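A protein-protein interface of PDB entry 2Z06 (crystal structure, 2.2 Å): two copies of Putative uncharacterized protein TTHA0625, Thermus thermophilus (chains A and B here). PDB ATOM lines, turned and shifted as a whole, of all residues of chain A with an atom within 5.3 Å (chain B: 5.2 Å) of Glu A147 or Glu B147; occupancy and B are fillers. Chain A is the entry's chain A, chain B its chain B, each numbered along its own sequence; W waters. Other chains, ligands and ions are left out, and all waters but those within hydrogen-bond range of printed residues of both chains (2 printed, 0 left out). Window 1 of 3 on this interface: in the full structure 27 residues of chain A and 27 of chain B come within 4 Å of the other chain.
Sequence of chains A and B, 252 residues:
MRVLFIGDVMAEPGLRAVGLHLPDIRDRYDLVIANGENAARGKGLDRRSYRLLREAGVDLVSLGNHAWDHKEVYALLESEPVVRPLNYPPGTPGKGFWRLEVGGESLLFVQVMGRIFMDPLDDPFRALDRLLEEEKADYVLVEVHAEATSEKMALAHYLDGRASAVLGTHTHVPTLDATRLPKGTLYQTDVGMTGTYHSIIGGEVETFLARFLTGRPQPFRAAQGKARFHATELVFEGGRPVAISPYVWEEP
OG1 of Thr A149 is in hydrogen-bond range of O of Thr B171, 3.4 Å away.
OG1 of Thr B149 sits at hydrogen-bond distance from O of Thr A171, 3.1 Å away.
The side-chain carboxylate of Glu B147 lies close to the side-chain carboxylate of Glu A147 (3.1 Å).
The backbone NH of Glu A147 sits at hydrogen-bond distance from the side-chain sulfur of Met A118.
SD of Met B118 lies within hydrogen-bond range of N of Glu B147.
OE1 of Glu B147 is in hydrogen-bond range of NE2 of His B170, at 3.4 Å.
Among the printed residues, pairs that only touch across the chains: Phe A117 with Phe B117 (3.7 Å), Phe A117 with Glu B147 (3.96 Å) and Glu A147 with Phe B117 (3.5 Å).
His A145 touches none of the printed residues of chain B.
Of chain B, only Phe B117 and Glu B147 come within 4 Å of Glu A147.
Of the printed residues of chain B, Thr A149 touches Thr B171.
Of the printed residues of chain A, Phe B117 touches Phe A117 (3.7 Å) and Glu A147 (3.5 Å).
Ala B146 touches none of the printed residues of chain A.
Glu B147 touches just these residues of chain A: Phe A117 (3.96 Å) and Glu A147 (3.1 Å).
Printed residues of chain A within 4 Å of Thr B171: Thr A149.
The nearest residue of chain B that does not touch Glu A147 is Ala B148 (4.5 Å).
The nearest residue of chain A that does not touch Glu B147 is Ala A148 (4.04 Å).
Of the 11 printed residues of chain A, 4 touch a printed residue of chain B.
Hydrophobic or aromatic side chains of chain A within 4 Å of the printed part of chain B: Phe A117.
Of the 11 printed residues of chain B, 4 touch a printed residue of chain A.
Printed residues of chain B that touch a printed residue of chain A: Phe B117, Glu B147, Thr B149 and Thr B171.
Among the printed residues, 6 pairs touch across the chains.
Among the printed residues, no Asp or Glu carboxylate lies within 4 Å of a Lys or Arg side-chain nitrogen of the other chain.
Phe A117 touches its own counterpart, Phe B117.
Phe A117 touches Glu B147, and with the chains exchanged Glu A147 touches Phe B117.
Glu A147 touches its own counterpart, Glu B147.
Thr A149 touches Thr B171, and with the chains exchanged Thr A171 touches Thr B149.
Positions printed for both chains: 116, 117, 118, 145, 146, 147, 148, 149, 152, 170 and 171.
Of the 6 pairs that touch across the chains among the printed residues, 6 have their exchanged pair printed and touching as well.
Water W2 lies within hydrogen-bond range of the side-chain carboxylate (OE2) of Glu B147 (2.8 Å) and the backbone NH (N) of Thr A149 (2.8 Å).
Water W1 lies within hydrogen-bond range of the side-chain carboxylate (OE2) of Glu B147, the backbone carbonyl oxygen (O) of Glu A147 and the side-chain hydroxyl (OG1) of Thr B171.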
ATOM      1  N   ILE A 116     -24.180   2.473 -18.162  1.00  0.00           N
ATOM      2  CA  ILE A 116     -23.990   1.560 -19.293  1.00  0.00           C
ATOM      3  C   ILE A 116     -24.598   0.190 -18.967  1.00  0.00           C
ATOM      4  O   ILE A 116     -24.245  -0.429 -17.960  1.00  0.00           O
ATOM      5  CB  ILE A 116     -22.488   1.372 -19.628  1.00  0.00           C
ATOM      6  CG1 ILE A 116     -21.853   2.722 -19.948  1.00  0.00           C
ATOM      7  CG2 ILE A 116     -22.323   0.410 -20.811  1.00  0.00           C
ATOM      8  CD1 ILE A 116     -22.560   3.473 -21.047  1.00  0.00           C
ATOM      9  N   PHE A 117     -25.502  -0.269 -19.837  1.00  0.00           N
ATOM     10  CA  PHE A 117     -26.202  -1.545 -19.681  1.00  0.00           C
ATOM     11  C   PHE A 117     -27.100  -1.515 -18.456  1.00  0.00           C
ATOM     12  O   PHE A 117     -27.447  -2.554 -17.904  1.00  0.00           O
ATOM     13  CB  PHE A 117     -25.219  -2.718 -19.561  1.00  0.00           C
ATOM     14  CG  PHE A 117     -24.274  -2.826 -20.706  1.00  0.00           C
ATOM     15  CD1 PHE A 117     -24.727  -2.678 -22.013  1.00  0.00           C
ATOM     16  CD2 PHE A 117     -22.918  -3.043 -20.488  1.00  0.00           C
ATOM     17  CE1 PHE A 117     -23.839  -2.742 -23.081  1.00  0.00           C
ATOM     18  CE2 PHE A 117     -22.031  -3.106 -21.550  1.00  0.00           C
ATOM     19  CZ  PHE A 117     -22.488  -2.955 -22.842  1.00  0.00           C
ATOM     20  N   MET A 118     -27.474  -0.310 -18.039  1.00  0.00           N
ATOM     21  CA  MET A 118     -28.330  -0.141 -16.879  1.00  0.00           C
ATOM     22  C   MET A 118     -29.371   0.936 -17.150  1.00  0.00           C
ATOM     23  O   MET A 118     -29.472   1.442 -18.260  1.00  0.00           O
ATOM     24  CB  MET A 118     -27.473   0.202 -15.659  1.00  0.00           C
ATOM     25  CG  MET A 118     -26.593  -0.966 -15.224  1.00  0.00           C
ATOM     26  SD  MET A 118     -25.438  -0.610 -13.891  1.00  0.00           S
ATOM     27  CE  MET A 118     -26.416  -1.074 -12.430  1.00  0.00           C
ATOM     28  N   HIS A 145     -21.539   1.141  -8.294  1.00  0.00           N
ATOM     29  CA  HIS A 145     -22.395   0.012  -8.627  1.00  0.00           C
ATOM     30  C   HIS A 145     -22.641   0.089 -10.124  1.00  0.00           C
ATOM     31  O   HIS A 145     -23.499   0.848 -10.580  1.00  0.00           O
ATOM     32  CB  HIS A 145     -23.710   0.122  -7.862  1.00  0.00           C
ATOM     33  CG  HIS A 145     -24.406  -1.186  -7.669  1.00  0.00           C
ATOM     34  ND1 HIS A 145     -25.522  -1.550  -8.389  1.00  0.00           N
ATOM     35  CD2 HIS A 145     -24.128  -2.229  -6.851  1.00  0.00           C
ATOM     36  CE1 HIS A 145     -25.901  -2.762  -8.022  1.00  0.00           C
ATOM     37  NE2 HIS A 145     -25.072  -3.196  -7.091  1.00  0.00           N
ATOM     38  N   ALA A 146     -21.880  -0.695 -10.886  1.00  0.00           N
ATOM     39  CA  ALA A 146     -22.011  -0.670 -12.333  1.00  0.00           C
ATOM     40  C   ALA A 146     -21.693  -1.990 -13.022  1.00  0.00           C
ATOM     41  O   ALA A 146     -21.021  -2.870 -12.475  1.00  0.00           O
ATOM     42  CB  ALA A 146     -21.127   0.428 -12.900  1.00  0.00           C
ATOM     43  N   GLU A 147     -22.177  -2.102 -14.249  1.00  0.00           N
ATOM     44  CA  GLU A 147     -21.965  -3.287 -15.054  1.00  0.00           C
ATOM     45  C   GLU A 147     -20.623  -3.219 -15.783  1.00  0.00           C
ATOM     46  O   GLU A 147     -19.799  -4.126 -15.668  1.00  0.00           O
ATOM     47  CB  GLU A 147     -23.083  -3.403 -16.085  1.00  0.00           C
ATOM     48  CG  GLU A 147     -23.836  -4.718 -16.071  1.00  0.00           C
ATOM     49  CD  GLU A 147     -23.011  -5.857 -16.588  1.00  0.00           C
ATOM     50  OE1 GLU A 147     -22.324  -5.653 -17.611  1.00  0.00           O
ATOM     51  OE2 GLU A 147     -23.059  -6.953 -15.991  1.00  0.00           O
ATOM     52  N   ALA A 148     -20.404  -2.127 -16.517  1.00  0.00           N
ATOM     53  CA  ALA A 148     -19.197  -1.980 -17.321  1.00  0.00           C
ATOM     54  C   ALA A 148     -17.908  -1.593 -16.608  1.00  0.00           C
ATOM     55  O   ALA A 148     -17.853  -0.635 -15.831  1.00  0.00           O
ATOM     56  CB  ALA A 148     -19.469  -1.020 -18.467  1.00  0.00           C
ATOM     57  N   THR A 149     -16.862  -2.358 -16.897  1.00  0.00           N
ATOM     58  CA  THR A 149     -15.551  -2.123 -16.318  1.00  0.00           C
ATOM     59  C   THR A 149     -15.015  -0.755 -16.741  1.00  0.00           C
ATOM     60  O   THR A 149     -14.390  -0.053 -15.956  1.00  0.00           O
ATOM     61  CB  THR A 149     -14.538  -3.215 -16.767  1.00  0.00           C
ATOM     62  OG1 THR A 149     -14.568  -3.337 -18.196  1.00  0.00           O
ATOM     63  CG2 THR A 149     -14.882  -4.564 -16.139  1.00  0.00           C
ATOM     64  N   LYS A 152     -16.540   1.962 -14.549  1.00  0.00           N
ATOM     65  CA  LYS A 152     -15.996   1.974 -13.202  1.00  0.00           C
ATOM     66  C   LYS A 152     -14.600   2.600 -13.238  1.00  0.00           C
ATOM     67  O   LYS A 152     -14.258   3.436 -12.403  1.00  0.00           O
ATOM     68  CB  LYS A 152     -15.918   0.549 -12.642  1.00  0.00           C
ATOM     69  CG  LYS A 152     -17.278  -0.066 -12.307  1.00  0.00           C
ATOM     70  CD  LYS A 152     -17.123  -1.501 -11.839  1.00  0.00           C
ATOM     71  CE  LYS A 152     -18.449  -2.079 -11.376  1.00  0.00           C
ATOM     72  NZ  LYS A 152     -18.295  -3.481 -10.902  1.00  0.00           N
ATOM     73  N   HIS A 170     -21.786  -4.853  -7.996  1.00  0.00           N
ATOM     74  CA  HIS A 170     -22.814  -5.244  -8.966  1.00  0.00           C
ATOM     75  C   HIS A 170     -22.514  -6.497  -9.793  1.00  0.00           C
ATOM     76  O   HIS A 170     -23.427  -7.228 -10.171  1.00  0.00           O
ATOM     77  CB  HIS A 170     -23.132  -4.072  -9.907  1.00  0.00           C
ATOM     78  CG  HIS A 170     -24.136  -4.397 -10.965  1.00  0.00           C
ATOM     79  ND1 HIS A 170     -25.443  -4.721 -10.676  1.00  0.00           N
ATOM     80  CD2 HIS A 170     -24.025  -4.451 -12.314  1.00  0.00           C
ATOM     81  CE1 HIS A 170     -26.096  -4.958 -11.801  1.00  0.00           C
ATOM     82  NE2 HIS A 170     -25.257  -4.800 -12.810  1.00  0.00           N
ATOM     83  N   THR A 171     -21.235  -6.741 -10.057  1.00  0.00           N
ATOM     84  CA  THR A 171     -20.786  -7.875 -10.858  1.00  0.00           C
ATOM     85  C   THR A 171     -20.812  -9.222 -10.131  1.00  0.00           C
ATOM     86  O   THR A 171     -20.946 -10.274 -10.766  1.00  0.00           O
ATOM     87  CB  THR A 171     -19.370  -7.571 -11.387  1.00  0.00           C
ATOM     88  OG1 THR A 171     -19.484  -6.788 -12.582  1.00  0.00           O
ATOM     89  CG2 THR A 171     -18.588  -8.826 -11.651  1.00  0.00           C
ATOM     90  N   ILE B 116     -25.946 -11.537 -23.884  1.00  0.00           N
ATOM     91  CA  ILE B 116     -26.445 -10.483 -22.997  1.00  0.00           C
ATOM     92  C   ILE B 116     -25.559  -9.243 -23.130  1.00  0.00           C
ATOM     93  O   ILE B 116     -24.342  -9.330 -23.050  1.00  0.00           O
ATOM     94  CB  ILE B 116     -26.458 -10.917 -21.512  1.00  0.00           C
ATOM     95  CG1 ILE B 116     -27.225 -12.241 -21.358  1.00  0.00           C
ATOM     96  CG2 ILE B 116     -27.068  -9.790 -20.646  1.00  0.00           C
ATOM     97  CD1 ILE B 116     -28.630 -12.249 -21.987  1.00  0.00           C
ATOM     98  N   PHE B 117     -26.185  -8.091 -23.348  1.00  0.00           N
ATOM     99  CA  PHE B 117     -25.472  -6.828 -23.516  1.00  0.00           C
ATOM    100  C   PHE B 117     -24.561  -6.841 -24.727  1.00  0.00           C
ATOM    101  O   PHE B 117     -23.664  -6.001 -24.834  1.00  0.00           O
ATOM    102  CB  PHE B 117     -24.632  -6.485 -22.287  1.00  0.00           C
ATOM    103  CG  PHE B 117     -25.416  -6.404 -21.022  1.00  0.00           C
ATOM    104  CD1 PHE B 117     -26.655  -5.770 -20.996  1.00  0.00           C
ATOM    105  CD2 PHE B 117     -24.915  -6.952 -19.848  1.00  0.00           C
ATOM    106  CE1 PHE B 117     -27.384  -5.685 -19.818  1.00  0.00           C
ATOM    107  CE2 PHE B 117     -25.628  -6.874 -18.666  1.00  0.00           C
ATOM    108  CZ  PHE B 117     -26.868  -6.240 -18.647  1.00  0.00           C
ATOM    109  N   MET B 118     -24.780  -7.799 -25.625  1.00  0.00           N
ATOM    110  CA  MET B 118     -23.978  -7.902 -26.833  1.00  0.00           C
ATOM    111  C   MET B 118     -24.868  -8.070 -28.056  1.00  0.00           C
ATOM    112  O   MET B 118     -26.090  -7.969 -27.965  1.00  0.00           O
ATOM    113  CB  MET B 118     -22.995  -9.063 -26.715  1.00  0.00           C
ATOM    114  CG  MET B 118     -22.155  -8.977 -25.460  1.00  0.00           C
ATOM    115  SD  MET B 118     -20.959 -10.294 -25.289  1.00  0.00           S
ATOM    116  CE  MET B 118     -19.470  -9.452 -25.800  1.00  0.00           C
ATOM    117  N   HIS B 145     -16.566 -15.640 -24.356  1.00  0.00           N
ATOM    118  CA  HIS B 145     -16.289 -14.219 -24.546  1.00  0.00           C
ATOM    119  C   HIS B 145     -17.594 -13.457 -24.315  1.00  0.00           C
ATOM    120  O   HIS B 145     -18.387 -13.256 -25.240  1.00  0.00           O
ATOM    121  CB  HIS B 145     -15.776 -14.026 -25.972  1.00  0.00           C
ATOM    122  CG  HIS B 145     -15.068 -12.732 -26.194  1.00  0.00           C
ATOM    123  ND1 HIS B 145     -15.653 -11.668 -26.845  1.00  0.00           N
ATOM    124  CD2 HIS B 145     -13.826 -12.325 -25.842  1.00  0.00           C
ATOM    125  CE1 HIS B 145     -14.800 -10.661 -26.884  1.00  0.00           C
ATOM    126  NE2 HIS B 145     -13.686 -11.033 -26.282  1.00  0.00           N
ATOM    127  N   ALA B 146     -17.815 -13.027 -23.082  1.00  0.00           N
ATOM    128  CA  ALA B 146     -19.069 -12.359 -22.747  1.00  0.00           C
ATOM    129  C   ALA B 146     -18.965 -11.196 -21.776  1.00  0.00           C
ATOM    130  O   ALA B 146     -17.943 -11.002 -21.112  1.00  0.00           O
ATOM    131  CB  ALA B 146     -20.050 -13.391 -22.189  1.00  0.00           C
ATOM    132  N   GLU B 147     -20.052 -10.434 -21.684  1.00  0.00           N
ATOM    133  CA  GLU B 147     -20.105  -9.292 -20.778  1.00  0.00           C
ATOM    134  C   GLU B 147     -20.710  -9.662 -19.424  1.00  0.00           C
ATOM    135  O   GLU B 147     -20.225  -9.236 -18.373  1.00  0.00           O
ATOM    136  CB  GLU B 147     -20.940  -8.169 -21.397  1.00  0.00           C
ATOM    137  CG  GLU B 147     -21.120  -6.957 -20.501  1.00  0.00           C
ATOM    138  CD  GLU B 147     -19.835  -6.170 -20.326  1.00  0.00           C
ATOM    139  OE1 GLU B 147     -18.977  -6.247 -21.230  1.00  0.00           O
ATOM    140  OE2 GLU B 147     -19.691  -5.462 -19.303  1.00  0.00           O
ATOM    141  N   ALA B 148     -21.770 -10.459 -19.458  1.00  0.00           N
ATOM    142  CA  ALA B 148     -22.480 -10.828 -18.244  1.00  0.00           C
ATOM    143  C   ALA B 148     -21.922 -12.014 -17.477  1.00  0.00           C
ATOM    144  O   ALA B 148     -21.769 -13.109 -18.014  1.00  0.00           O
ATOM    145  CB  ALA B 148     -23.928 -11.073 -18.571  1.00  0.00           C
ATOM    146  N   THR B 149     -21.636 -11.786 -16.203  1.00  0.00           N
ATOM    147  CA  THR B 149     -21.119 -12.841 -15.348  1.00  0.00           C
ATOM    148  C   THR B 149     -22.138 -13.986 -15.244  1.00  0.00           C
ATOM    149  O   THR B 149     -21.762 -15.156 -15.224  1.00  0.00           O
ATOM    150  CB  THR B 149     -20.763 -12.278 -13.945  1.00  0.00           C
ATOM    151  OG1 THR B 149     -21.869 -11.539 -13.416  1.00  0.00           O
ATOM    152  CG2 THR B 149     -19.576 -11.325 -14.053  1.00  0.00           C
ATOM    153  N   LYS B 152     -21.849 -16.193 -18.305  1.00  0.00           N
ATOM    154  CA  LYS B 152     -20.630 -16.992 -18.222  1.00  0.00           C
ATOM    155  C   LYS B 152     -20.824 -18.138 -17.215  1.00  0.00           C
ATOM    156  O   LYS B 152     -20.442 -19.277 -17.482  1.00  0.00           O
ATOM    157  CB  LYS B 152     -19.462 -16.121 -17.793  1.00  0.00           C
ATOM    158  CG  LYS B 152     -18.976 -15.186 -18.869  1.00  0.00           C
ATOM    159  CD  LYS B 152     -17.817 -14.374 -18.343  1.00  0.00           C
ATOM    160  CE  LYS B 152     -17.121 -13.601 -19.446  1.00  0.00           C
ATOM    161  NZ  LYS B 152     -15.995 -12.816 -18.864  1.00  0.00           N
ATOM    162  N   HIS B 170     -13.148 -11.017 -22.420  1.00  0.00           N
ATOM    163  CA  HIS B 170     -13.914  -9.841 -22.849  1.00  0.00           C
ATOM    164  C   HIS B 170     -13.955  -8.712 -21.821  1.00  0.00           C
ATOM    165  O   HIS B 170     -13.796  -7.552 -22.168  1.00  0.00           O
ATOM    166  CB  HIS B 170     -15.353 -10.213 -23.219  1.00  0.00           C
ATOM    167  CG  HIS B 170     -16.160  -9.063 -23.734  1.00  0.00           C
ATOM    168  ND1 HIS B 170     -15.825  -8.375 -24.879  1.00  0.00           N
ATOM    169  CD2 HIS B 170     -17.292  -8.484 -23.268  1.00  0.00           C
ATOM    170  CE1 HIS B 170     -16.716  -7.424 -25.101  1.00  0.00           C
ATOM    171  NE2 HIS B 170     -17.617  -7.470 -24.137  1.00  0.00           N
ATOM    172  N   THR B 171     -14.168  -9.060 -20.561  1.00  0.00           N
ATOM    173  CA  THR B 171     -14.243  -8.083 -19.478  1.00  0.00           C
ATOM    174  C   THR B 171     -12.932  -7.333 -19.163  1.00  0.00           C
ATOM    175  O   THR B 171     -12.947  -6.251 -18.556  1.00  0.00           O
ATOM    176  CB  THR B 171     -14.816  -8.785 -18.217  1.00  0.00           C
ATOM    177  OG1 THR B 171     -16.216  -8.498 -18.135  1.00  0.00           O
ATOM    178  CG2 THR B 171     -14.114  -8.351 -16.956  1.00  0.00           C
HETATM  179  O   HOH W   1     -19.104  -6.971 -16.908  1.00  0.00           O
HETATM  180  O   HOH W   2     -17.242  -4.847 -18.172  1.00  0.00           O
